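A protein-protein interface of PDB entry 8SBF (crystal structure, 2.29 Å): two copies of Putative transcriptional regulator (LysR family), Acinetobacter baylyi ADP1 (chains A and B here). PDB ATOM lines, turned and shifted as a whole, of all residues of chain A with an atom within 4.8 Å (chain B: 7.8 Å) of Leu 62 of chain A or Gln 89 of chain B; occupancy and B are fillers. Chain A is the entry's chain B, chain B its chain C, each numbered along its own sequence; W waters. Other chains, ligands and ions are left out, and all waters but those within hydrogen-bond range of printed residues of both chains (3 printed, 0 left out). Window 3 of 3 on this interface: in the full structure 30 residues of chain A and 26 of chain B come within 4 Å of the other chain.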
ATOM      1  N   ALA A  47      13.406  11.001  -6.705  1.00  0.00           N
ATOM      2  CA  ALA A  47      12.911  11.539  -5.446  1.00  0.00           C
ATOM      3  C   ALA A  47      12.138  10.438  -4.728  1.00  0.00           C
ATOM      4  O   ALA A  47      11.643   9.509  -5.371  1.00  0.00           O
ATOM      5  CB  ALA A  47      12.010  12.764  -5.673  1.00  0.00           C
ATOM      6  N   PRO A  48      12.031  10.520  -3.404  1.00  0.00           N
ATOM      7  CA  PRO A  48      11.206   9.555  -2.672  1.00  0.00           C
ATOM      8  C   PRO A  48       9.725   9.846  -2.858  1.00  0.00           C
ATOM      9  O   PRO A  48       9.312  10.971  -3.150  1.00  0.00           O
ATOM     10  CB  PRO A  48      11.632   9.752  -1.213  1.00  0.00           C
ATOM     11  CG  PRO A  48      12.071  11.180  -1.151  1.00  0.00           C
ATOM     12  CD  PRO A  48      12.681  11.491  -2.501  1.00  0.00           C
ATOM     13  N   LEU A  49       8.918   8.801  -2.683  1.00  0.00           N
ATOM     14  CA  LEU A  49       7.470   8.917  -2.771  1.00  0.00           C
ATOM     15  C   LEU A  49       6.788   8.918  -1.408  1.00  0.00           C
ATOM     16  O   LEU A  49       5.602   9.261  -1.328  1.00  0.00           O
ATOM     17  CB  LEU A  49       6.899   7.774  -3.619  1.00  0.00           C
ATOM     18  CG  LEU A  49       7.243   7.821  -5.108  1.00  0.00           C
ATOM     19  CD1 LEU A  49       6.765   6.562  -5.810  1.00  0.00           C
ATOM     20  CD2 LEU A  49       6.635   9.055  -5.757  1.00  0.00           C
ATOM     21  N   ASN A  60       4.264  11.476   0.523  1.00  0.00           N
ATOM     22  CA  ASN A  60       4.743  12.847   0.555  1.00  0.00           C
ATOM     23  C   ASN A  60       4.059  13.646  -0.554  1.00  0.00           C
ATOM     24  O   ASN A  60       3.219  13.133  -1.298  1.00  0.00           O
ATOM     25  CB  ASN A  60       6.269  12.894   0.433  1.00  0.00           C
ATOM     26  CG  ASN A  60       6.778  12.310  -0.870  1.00  0.00           C
ATOM     27  OD1 ASN A  60       6.043  12.199  -1.850  1.00  0.00           O
ATOM     28  ND2 ASN A  60       8.053  11.937  -0.884  1.00  0.00           N
ATOM     29  N   ASP A  61       4.433  14.923  -0.663  1.00  0.00           N
ATOM     30  CA  ASP A  61       3.778  15.817  -1.615  1.00  0.00           C
ATOM     31  C   ASP A  61       3.755  15.221  -3.017  1.00  0.00           C
ATOM     32  O   ASP A  61       2.720  15.228  -3.694  1.00  0.00           O
ATOM     33  CB  ASP A  61       4.488  17.172  -1.616  1.00  0.00           C
ATOM     34  CG  ASP A  61       3.811  18.184  -2.517  1.00  0.00           C
ATOM     35  OD1 ASP A  61       2.647  18.548  -2.239  1.00  0.00           O
ATOM     36  OD2 ASP A  61       4.444  18.621  -3.501  1.00  0.00           O
ATOM     37  N   LEU A  62       4.893  14.695  -3.474  1.00  0.00           N
ATOM     38  CA  LEU A  62       4.946  14.096  -4.805  1.00  0.00           C
ATOM     39  C   LEU A  62       4.151  12.799  -4.855  1.00  0.00           C
ATOM     40  O   LEU A  62       3.443  12.535  -5.834  1.00  0.00           O
ATOM     41  CB  LEU A  62       6.399  13.855  -5.208  1.00  0.00           C
ATOM     42  CG  LEU A  62       6.644  13.147  -6.544  1.00  0.00           C
ATOM     43  CD1 LEU A  62       6.120  13.965  -7.711  1.00  0.00           C
ATOM     44  CD2 LEU A  62       8.133  12.859  -6.714  1.00  0.00           C
ATOM     45  N   GLY A  63       4.251  11.975  -3.809  1.00  0.00           N
ATOM     46  CA  GLY A  63       3.495  10.732  -3.787  1.00  0.00           C
ATOM     47  C   GLY A  63       1.998  10.956  -3.857  1.00  0.00           C
ATOM     48  O   GLY A  63       1.290  10.256  -4.587  1.00  0.00           O
ATOM     49  N   ARG A  64       1.490  11.929  -3.094  1.00  0.00           N
ATOM     50  CA  ARG A  64       0.064  12.236  -3.152  1.00  0.00           C
ATOM     51  C   ARG A  64      -0.354  12.627  -4.562  1.00  0.00           C
ATOM     52  O   ARG A  64      -1.447  12.273  -5.015  1.00  0.00           O
ATOM     53  CB  ARG A  64      -0.281  13.357  -2.172  1.00  0.00           C
ATOM     54  CG  ARG A  64      -0.474  12.907  -0.737  1.00  0.00           C
ATOM     55  CD  ARG A  64      -1.352  13.892   0.027  1.00  0.00           C
ATOM     56  NE  ARG A  64      -1.027  15.279  -0.299  1.00  0.00           N
ATOM     57  CZ  ARG A  64      -0.043  15.970   0.259  1.00  0.00           C
ATOM     58  NH1 ARG A  64       0.743  15.435   1.180  1.00  0.00           N
ATOM     59  NH2 ARG A  64       0.158  17.231  -0.118  1.00  0.00           N
ATOM     60  N   PHE A  65       0.504  13.365  -5.269  1.00  0.00           N
ATOM     61  CA  PHE A  65       0.160  13.816  -6.614  1.00  0.00           C
ATOM     62  C   PHE A  65       0.180  12.663  -7.607  1.00  0.00           C
ATOM     63  O   PHE A  65      -0.650  12.612  -8.523  1.00  0.00           O
ATOM     64  CB  PHE A  65       1.124  14.918  -7.053  1.00  0.00           C
ATOM     65  CG  PHE A  65       0.903  15.394  -8.460  1.00  0.00           C
ATOM     66  CD1 PHE A  65      -0.111  16.291  -8.750  1.00  0.00           C
ATOM     67  CD2 PHE A  65       1.712  14.949  -9.490  1.00  0.00           C
ATOM     68  CE1 PHE A  65      -0.316  16.732 -10.043  1.00  0.00           C
ATOM     69  CE2 PHE A  65       1.513  15.386 -10.785  1.00  0.00           C
ATOM     70  CZ  PHE A  65       0.498  16.279 -11.062  1.00  0.00           C
ATOM     71  N   LEU A  66       1.113  11.725  -7.442  1.00  0.00           N
ATOM     72  CA  LEU A  66       1.281  10.640  -8.399  1.00  0.00           C
ATOM     73  C   LEU A  66       0.396   9.433  -8.114  1.00  0.00           C
ATOM     74  O   LEU A  66       0.118   8.661  -9.038  1.00  0.00           O
ATOM     75  CB  LEU A  66       2.741  10.179  -8.421  1.00  0.00           C
ATOM     76  CG  LEU A  66       3.763  11.142  -9.025  1.00  0.00           C
ATOM     77  CD1 LEU A  66       5.162  10.564  -8.883  1.00  0.00           C
ATOM     78  CD2 LEU A  66       3.445  11.427 -10.485  1.00  0.00           C
ATOM     79  N   PHE B  80       3.624   9.978 -16.179  1.00  0.00           N
ATOM     80  CA  PHE B  80       3.967   9.676 -14.792  1.00  0.00           C
ATOM     81  C   PHE B  80       5.447   9.935 -14.530  1.00  0.00           C
ATOM     82  O   PHE B  80       5.812  10.594 -13.550  1.00  0.00           O
ATOM     83  CB  PHE B  80       3.602   8.218 -14.488  1.00  0.00           C
ATOM     84  CG  PHE B  80       3.758   7.832 -13.042  1.00  0.00           C
ATOM     85  CD1 PHE B  80       4.998   7.495 -12.528  1.00  0.00           C
ATOM     86  CD2 PHE B  80       2.656   7.783 -12.204  1.00  0.00           C
ATOM     87  CE1 PHE B  80       5.139   7.134 -11.201  1.00  0.00           C
ATOM     88  CE2 PHE B  80       2.794   7.419 -10.877  1.00  0.00           C
ATOM     89  CZ  PHE B  80       4.035   7.095 -10.376  1.00  0.00           C
ATOM     90  N   GLU B  81       6.318   9.422 -15.405  1.00  0.00           N
ATOM     91  CA  GLU B  81       7.753   9.608 -15.209  1.00  0.00           C
ATOM     92  C   GLU B  81       8.147  11.074 -15.340  1.00  0.00           C
ATOM     93  O   GLU B  81       8.933  11.584 -14.533  1.00  0.00           O
ATOM     94  CB  GLU B  81       8.540   8.754 -16.204  1.00  0.00           C
ATOM     95  CG  GLU B  81       8.679   7.293 -15.803  1.00  0.00           C
ATOM     96  CD  GLU B  81       9.778   6.579 -16.573  1.00  0.00           C
ATOM     97  OE1 GLU B  81      10.345   7.186 -17.508  1.00  0.00           O
ATOM     98  OE2 GLU B  81      10.079   5.414 -16.238  1.00  0.00           O
ATOM     99  N   GLN B  82       7.624  11.763 -16.356  1.00  0.00           N
ATOM    100  CA  GLN B  82       7.966  13.171 -16.546  1.00  0.00           C
ATOM    101  C   GLN B  82       7.494  14.010 -15.365  1.00  0.00           C
ATOM    102  O   GLN B  82       8.235  14.858 -14.854  1.00  0.00           O
ATOM    103  CB  GLN B  82       7.359  13.684 -17.855  1.00  0.00           C
ATOM    104  CG  GLN B  82       7.511  15.184 -18.091  1.00  0.00           C
ATOM    105  CD  GLN B  82       8.944  15.597 -18.381  1.00  0.00           C
ATOM    106  OE1 GLN B  82       9.672  16.033 -17.488  1.00  0.00           O
ATOM    107  NE2 GLN B  82       9.356  15.466 -19.640  1.00  0.00           N
ATOM    108  N   ALA B  83       6.255  13.789 -14.917  1.00  0.00           N
ATOM    109  CA  ALA B  83       5.738  14.544 -13.781  1.00  0.00           C
ATOM    110  C   ALA B  83       6.614  14.354 -12.550  1.00  0.00           C
ATOM    111  O   ALA B  83       6.822  15.293 -11.773  1.00  0.00           O
ATOM    112  CB  ALA B  83       4.298  14.127 -13.484  1.00  0.00           C
ATOM    113  N   ALA B  84       7.142  13.143 -12.360  1.00  0.00           N
ATOM    114  CA  ALA B  84       8.013  12.887 -11.218  1.00  0.00           C
ATOM    115  C   ALA B  84       9.380  13.529 -11.417  1.00  0.00           C
ATOM    116  O   ALA B  84       9.877  14.243 -10.539  1.00  0.00           O
ATOM    117  CB  ALA B  84       8.151  11.382 -10.995  1.00  0.00           C
ATOM    118  N   LYS B  85      10.005  13.280 -12.570  1.00  0.00           N
ATOM    119  CA  LYS B  85      11.330  13.833 -12.833  1.00  0.00           C
ATOM    120  C   LYS B  85      11.300  15.356 -12.816  1.00  0.00           C
ATOM    121  O   LYS B  85      12.159  16.000 -12.203  1.00  0.00           O
ATOM    122  CB  LYS B  85      11.852  13.317 -14.175  1.00  0.00           C
ATOM    123  CG  LYS B  85      12.588  11.988 -14.086  1.00  0.00           C
ATOM    124  CD  LYS B  85      12.584  11.263 -15.424  1.00  0.00           C
ATOM    125  CE  LYS B  85      13.914  10.577 -15.698  1.00  0.00           C
ATOM    126  NZ  LYS B  85      14.239   9.528 -14.692  1.00  0.00           N
ATOM    127  N   GLY B  86      10.320  15.948 -13.487  1.00  0.00           N
ATOM    128  CA  GLY B  86      10.183  17.388 -13.514  1.00  0.00           C
ATOM    129  C   GLY B  86       9.536  17.998 -12.292  1.00  0.00           C
ATOM    130  O   GLY B  86       9.435  19.227 -12.209  1.00  0.00           O
ATOM    131  N   GLU B  87       9.106  17.176 -11.338  1.00  0.00           N
ATOM    132  CA  GLU B  87       8.389  17.641 -10.153  1.00  0.00           C
ATOM    133  C   GLU B  87       7.298  18.636 -10.548  1.00  0.00           C
ATOM    134  O   GLU B  87       7.316  19.813 -10.188  1.00  0.00           O
ATOM    135  CB  GLU B  87       9.359  18.246  -9.134  1.00  0.00           C
ATOM    136  CG  GLU B  87      10.143  17.202  -8.347  1.00  0.00           C
ATOM    137  CD  GLU B  87      11.239  17.806  -7.491  1.00  0.00           C
ATOM    138  OE1 GLU B  87      12.182  18.397  -8.056  1.00  0.00           O
ATOM    139  OE2 GLU B  87      11.155  17.696  -6.249  1.00  0.00           O
ATOM    140  N   LEU B  88       6.331  18.124 -11.315  1.00  0.00           N
ATOM    141  CA  LEU B  88       5.253  18.931 -11.871  1.00  0.00           C
ATOM    142  C   LEU B  88       4.020  18.964 -10.974  1.00  0.00           C
ATOM    143  O   LEU B  88       2.898  19.111 -11.477  1.00  0.00           O
ATOM    144  CB  LEU B  88       4.883  18.413 -13.260  1.00  0.00           C
ATOM    145  CG  LEU B  88       6.046  18.242 -14.241  1.00  0.00           C
ATOM    146  CD1 LEU B  88       5.549  17.743 -15.594  1.00  0.00           C
ATOM    147  CD2 LEU B  88       6.814  19.547 -14.400  1.00  0.00           C
ATOM    148  N   GLN B  89       4.197  18.838  -9.662  1.00  0.00           N
ATOM    149  CA  GLN B  89       3.055  18.867  -8.760  1.00  0.00           C
ATOM    150  C   GLN B  89       2.372  20.227  -8.796  1.00  0.00           C
ATOM    151  O   GLN B  89       2.993  21.259  -9.069  1.00  0.00           O
ATOM    152  CB  GLN B  89       3.488  18.564  -7.323  1.00  0.00           C
ATOM    153  CG  GLN B  89       4.232  17.266  -7.135  1.00  0.00           C
ATOM    154  CD  GLN B  89       5.722  17.476  -6.968  1.00  0.00           C
ATOM    155  OE1 GLN B  89       6.429  17.774  -7.929  1.00  0.00           O
ATOM    156  NE2 GLN B  89       6.208  17.325  -5.739  1.00  0.00           N
ATOM    157  N   SER B  90       1.074  20.223  -8.509  1.00  0.00           N
ATOM    158  CA  SER B  90       0.379  21.450  -8.173  1.00  0.00           C
ATOM    159  C   SER B  90       0.740  21.868  -6.748  1.00  0.00           C
ATOM    160  O   SER B  90       1.403  21.137  -6.005  1.00  0.00           O
ATOM    161  CB  SER B  90      -1.131  21.263  -8.317  1.00  0.00           C
ATOM    162  OG  SER B  90      -1.551  20.064  -7.690  1.00  0.00           O
ATOM    163  N   ILE B  91       0.304  23.064  -6.368  1.00  0.00           N
ATOM    164  CA  ILE B  91       0.511  23.548  -5.007  1.00  0.00           C
ATOM    165  C   ILE B  91      -0.567  22.941  -4.117  1.00  0.00           C
ATOM    166  O   ILE B  91      -1.764  23.093  -4.381  1.00  0.00           O
ATOM    167  CB  ILE B  91       0.483  25.081  -4.947  1.00  0.00           C
ATOM    168  CG1 ILE B  91       1.556  25.661  -5.871  1.00  0.00           C
ATOM    169  CG2 ILE B  91       0.697  25.559  -3.511  1.00  0.00           C
ATOM    170  CD1 ILE B  91       1.596  27.175  -5.898  1.00  0.00           C
ATOM    171  N   ASP B  92      -0.141  22.250  -3.058  1.00  0.00           N
ATOM    172  CA  ASP B  92      -1.061  21.583  -2.136  1.00  0.00           C
ATOM    173  C   ASP B  92      -0.381  21.579  -0.764  1.00  0.00           C
ATOM    174  O   ASP B  92       0.319  20.628  -0.410  1.00  0.00           O
ATOM    175  CB  ASP B  92      -1.397  20.177  -2.610  1.00  0.00           C
ATOM    176  CG  ASP B  92      -2.538  19.554  -1.833  1.00  0.00           C
ATOM    177  OD1 ASP B  92      -3.051  20.205  -0.899  1.00  0.00           O
ATOM    178  OD2 ASP B  92      -2.925  18.413  -2.160  1.00  0.00           O
ATOM    179  N   TYR B 278      10.124  15.557   2.501  1.00  0.00           N
ATOM    180  CA  TYR B 278      10.327  16.003   1.130  1.00  0.00           C
ATOM    181  C   TYR B 278       9.660  17.356   0.909  1.00  0.00           C
ATOM    182  O   TYR B 278       8.548  17.607   1.384  1.00  0.00           O
ATOM    183  CB  TYR B 278       9.767  14.969   0.153  1.00  0.00           C
ATOM    184  CG  TYR B 278       9.626  15.480  -1.262  1.00  0.00           C
ATOM    185  CD1 TYR B 278      10.689  15.423  -2.154  1.00  0.00           C
ATOM    186  CD2 TYR B 278       8.427  16.021  -1.708  1.00  0.00           C
ATOM    187  CE1 TYR B 278      10.562  15.890  -3.449  1.00  0.00           C
ATOM    188  CE2 TYR B 278       8.291  16.491  -2.999  1.00  0.00           C
ATOM    189  CZ  TYR B 278       9.361  16.424  -3.865  1.00  0.00           C
ATOM    190  OH  TYR B 278       9.226  16.892  -5.152  1.00  0.00           O
ATOM    191  N   GLN B 279      10.349  18.233   0.182  1.00  0.00           N
ATOM    192  CA  GLN B 279       9.868  19.579  -0.108  1.00  0.00           C
ATOM    193  C   GLN B 279       9.531  19.665  -1.591  1.00  0.00           C
ATOM    194  O   GLN B 279      10.428  19.615  -2.440  1.00  0.00           O
ATOM    195  CB  GLN B 279      10.910  20.627   0.277  1.00  0.00           C
ATOM    196  CG  GLN B 279      11.235  20.678   1.761  1.00  0.00           C
ATOM    197  CD  GLN B 279      12.138  21.843   2.118  1.00  0.00           C
ATOM    198  OE1 GLN B 279      12.679  22.517   1.241  1.00  0.00           O
ATOM    199  NE2 GLN B 279      12.307  22.087   3.414  1.00  0.00           N
ATOM    200  N   GLY B 280       8.245  19.799  -1.899  1.00  0.00           N
ATOM    201  CA  GLY B 280       7.806  19.923  -3.270  1.00  0.00           C
ATOM    202  C   GLY B 280       7.974  21.330  -3.791  1.00  0.00           C
ATOM    203  O   GLY B 280       8.344  22.269  -3.065  1.00  0.00           O
ATOM    204  N   PRO B 281       7.700  21.502  -5.087  1.00  0.00           N
ATOM    205  CA  PRO B 281       7.836  22.844  -5.684  1.00  0.00           C
ATOM    206  C   PRO B 281       6.885  23.863  -5.085  1.00  0.00           C
ATOM    207  O   PRO B 281       7.235  25.048  -4.994  1.00  0.00           O
ATOM    208  CB  PRO B 281       7.544  22.598  -7.172  1.00  0.00           C
ATOM    209  CG  PRO B 281       6.707  21.356  -7.196  1.00  0.00           C
ATOM    210  CD  PRO B 281       7.206  20.506  -6.054  1.00  0.00           C
ATOM    211  N   GLY B 282       5.689  23.443  -4.672  1.00  0.00           N
ATOM    212  CA  GLY B 282       4.762  24.381  -4.060  1.00  0.00           C
ATOM    213  C   GLY B 282       5.270  24.922  -2.739  1.00  0.00           C
ATOM    214  O   GLY B 282       5.166  26.121  -2.466  1.00  0.00           O
ATOM    215  N   LEU B 283       5.823  24.045  -1.896  1.00  0.00           N
ATOM    216  CA  LEU B 283       6.400  24.500  -0.638  1.00  0.00           C
ATOM    217  C   LEU B 283       7.567  25.447  -0.881  1.00  0.00           C
ATOM    218  O   LEU B 283       7.712  26.458  -0.184  1.00  0.00           O
ATOM    219  CB  LEU B 283       6.849  23.300   0.194  1.00  0.00           C
ATOM    220  CG  LEU B 283       7.671  23.601   1.450  1.00  0.00           C
ATOM    221  CD1 LEU B 283       6.881  24.450   2.430  1.00  0.00           C
ATOM    222  CD2 LEU B 283       8.124  22.304   2.106  1.00  0.00           C
HETATM  223  O   HOH W   1       2.518  21.713  -2.411  1.00  0.00           O
HETATM  224  O   HOH W   2       3.011  20.200  -0.207  1.00  0.00           O
HETATM  225  O   HOH W   3       3.707  21.108  -4.525  1.00  0.00           O
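OD2 of Asp 61 of chain A is in hydrogen-bond range of NE2 of Gln 89 of chain B, 3.1 Å away. The side-chain carboxylate of Asp 92 of chain B lies within salt-bridge range of the guanidinium group of Arg 64 of chain A, at 3.9 Å.
O of Ala 83 of chain B lies within hydrogen-bond range of N of Leu 88 of chain B (2.9 Å). OH of Tyr 278 of chain B is in hydrogen-bond range of NE2 of Gln 89 of chain B. The backbone carbonyl oxygen (O) of Pro 48 of chain A is in hydrogen-bond range of the side-chain amide nitrogen (ND2) of Asn 60 of chain A (2.8 Å). The side-chain amide oxygen (OD1) of Asn 60 of chain A lies close to the backbone carbonyl oxygen (O) of Leu 49 of chain A (3.0 Å). The backbone NH (N) of Gly 63 of chain A lies within hydrogen-bond range of the side-chain amide oxygen (OD1) of Asn 60 of chain A (2.7 Å). OD1 of Asp 61 of chain A is in salt-bridge range of NH2 of Arg 64 of chain A (3.5 Å).
Tyr 278 of chain B touches Asn 60 of chain A. Asp 92 of chain B touches Asp 61 of chain A. Gly 280 of chain B touches Asp 61 of chain A. Leu 62 of chain A touches Gln 89 of chain B (CB to NE2, 3.5 Å). Leu 62 of chain A touches Tyr 278 of chain B. Phe 65 of chain A touches Leu 88 of chain B (CZ to O, 3.7 Å). Gln 89 of chain B touches Phe 65 of chain A (CG to CB, 3.9 Å). Leu 66 of chain A touches Phe 80 of chain B (O to CE2, 3.5 Å). CB of Ala 84 of chain B touches CD1 of Leu 66 of chain A (3.8 Å).
Of chain A, only Asp 61, Leu 62 and Phe 65 come within 4 Å of Gln 89 of chain B. Of the printed residues of chain A, Tyr 278 of chain B touches Asn 60 (3.6 Å) and Leu 62 (3.9 Å). Of the printed residues of chain B, Asp 61 of chain A touches Gln 89 (3.1 Å), Asp 92 (3.6 Å) and Gly 280 (3.6 Å). Printed residues of chain A within 4 Å of Gly 280 of chain B: Asp 61 (3.6 Å). Of the printed residues of chain B, Asn 60 of chain A touches Tyr 278 (3.6 Å). Printed residues of chain B within 4 Å of Phe 65 of chain A: Leu 88 and Gln 89. The nearest printed residue of chain B that does not touch Asn 60 of chain A is Gln 89 of chain B (6.4 Å).
Of the 19 printed residues of chain B, 7 touch a printed residue of chain A. Along chain B the printed residues that touch a printed residue of chain A span positions 80 to 280. Printed residues of chain A that touch a printed residue of chain B: Asn 60, Asp 61, Leu 62, Arg 64, Phe 65 and Leu 66. Hydrophobic or aromatic side chains of chain A within 4 Å of the printed part of chain B: Leu 62, Phe 65 and Leu 66. Among the printed residues, 11 pairs touch across the chains. Among the printed residues, Asp or Glu carboxylates within 4 Å of a Lys or Arg side-chain nitrogen of the other chain: Arg 64 of chain A with Asp 92 of chain B (3.9 Å).
No position is printed for both chains. Of the 11 pairs that touch across the chains among the printed residues, none has its exchanged pair printed and touching as well.
Water W2 lies within hydrogen-bond range of the side-chain carboxylate (OD1) of Asp 61 of chain A (2.6 Å) and the backbone carbonyl oxygen (O) of Asp 92 of chain B (2.7 Å). Water W3 lies within hydrogen-bond range of O of Ser 90 of chain B, OD2 of Asp 61 of chain A and N of Gly 282 of chain B. Water W1 lies within hydrogen-bond range of the backbone NH of Asp 92 of chain B (2.8 Å) and the side-chain carboxylate of Asp 61 of chain A (3.2 Å).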
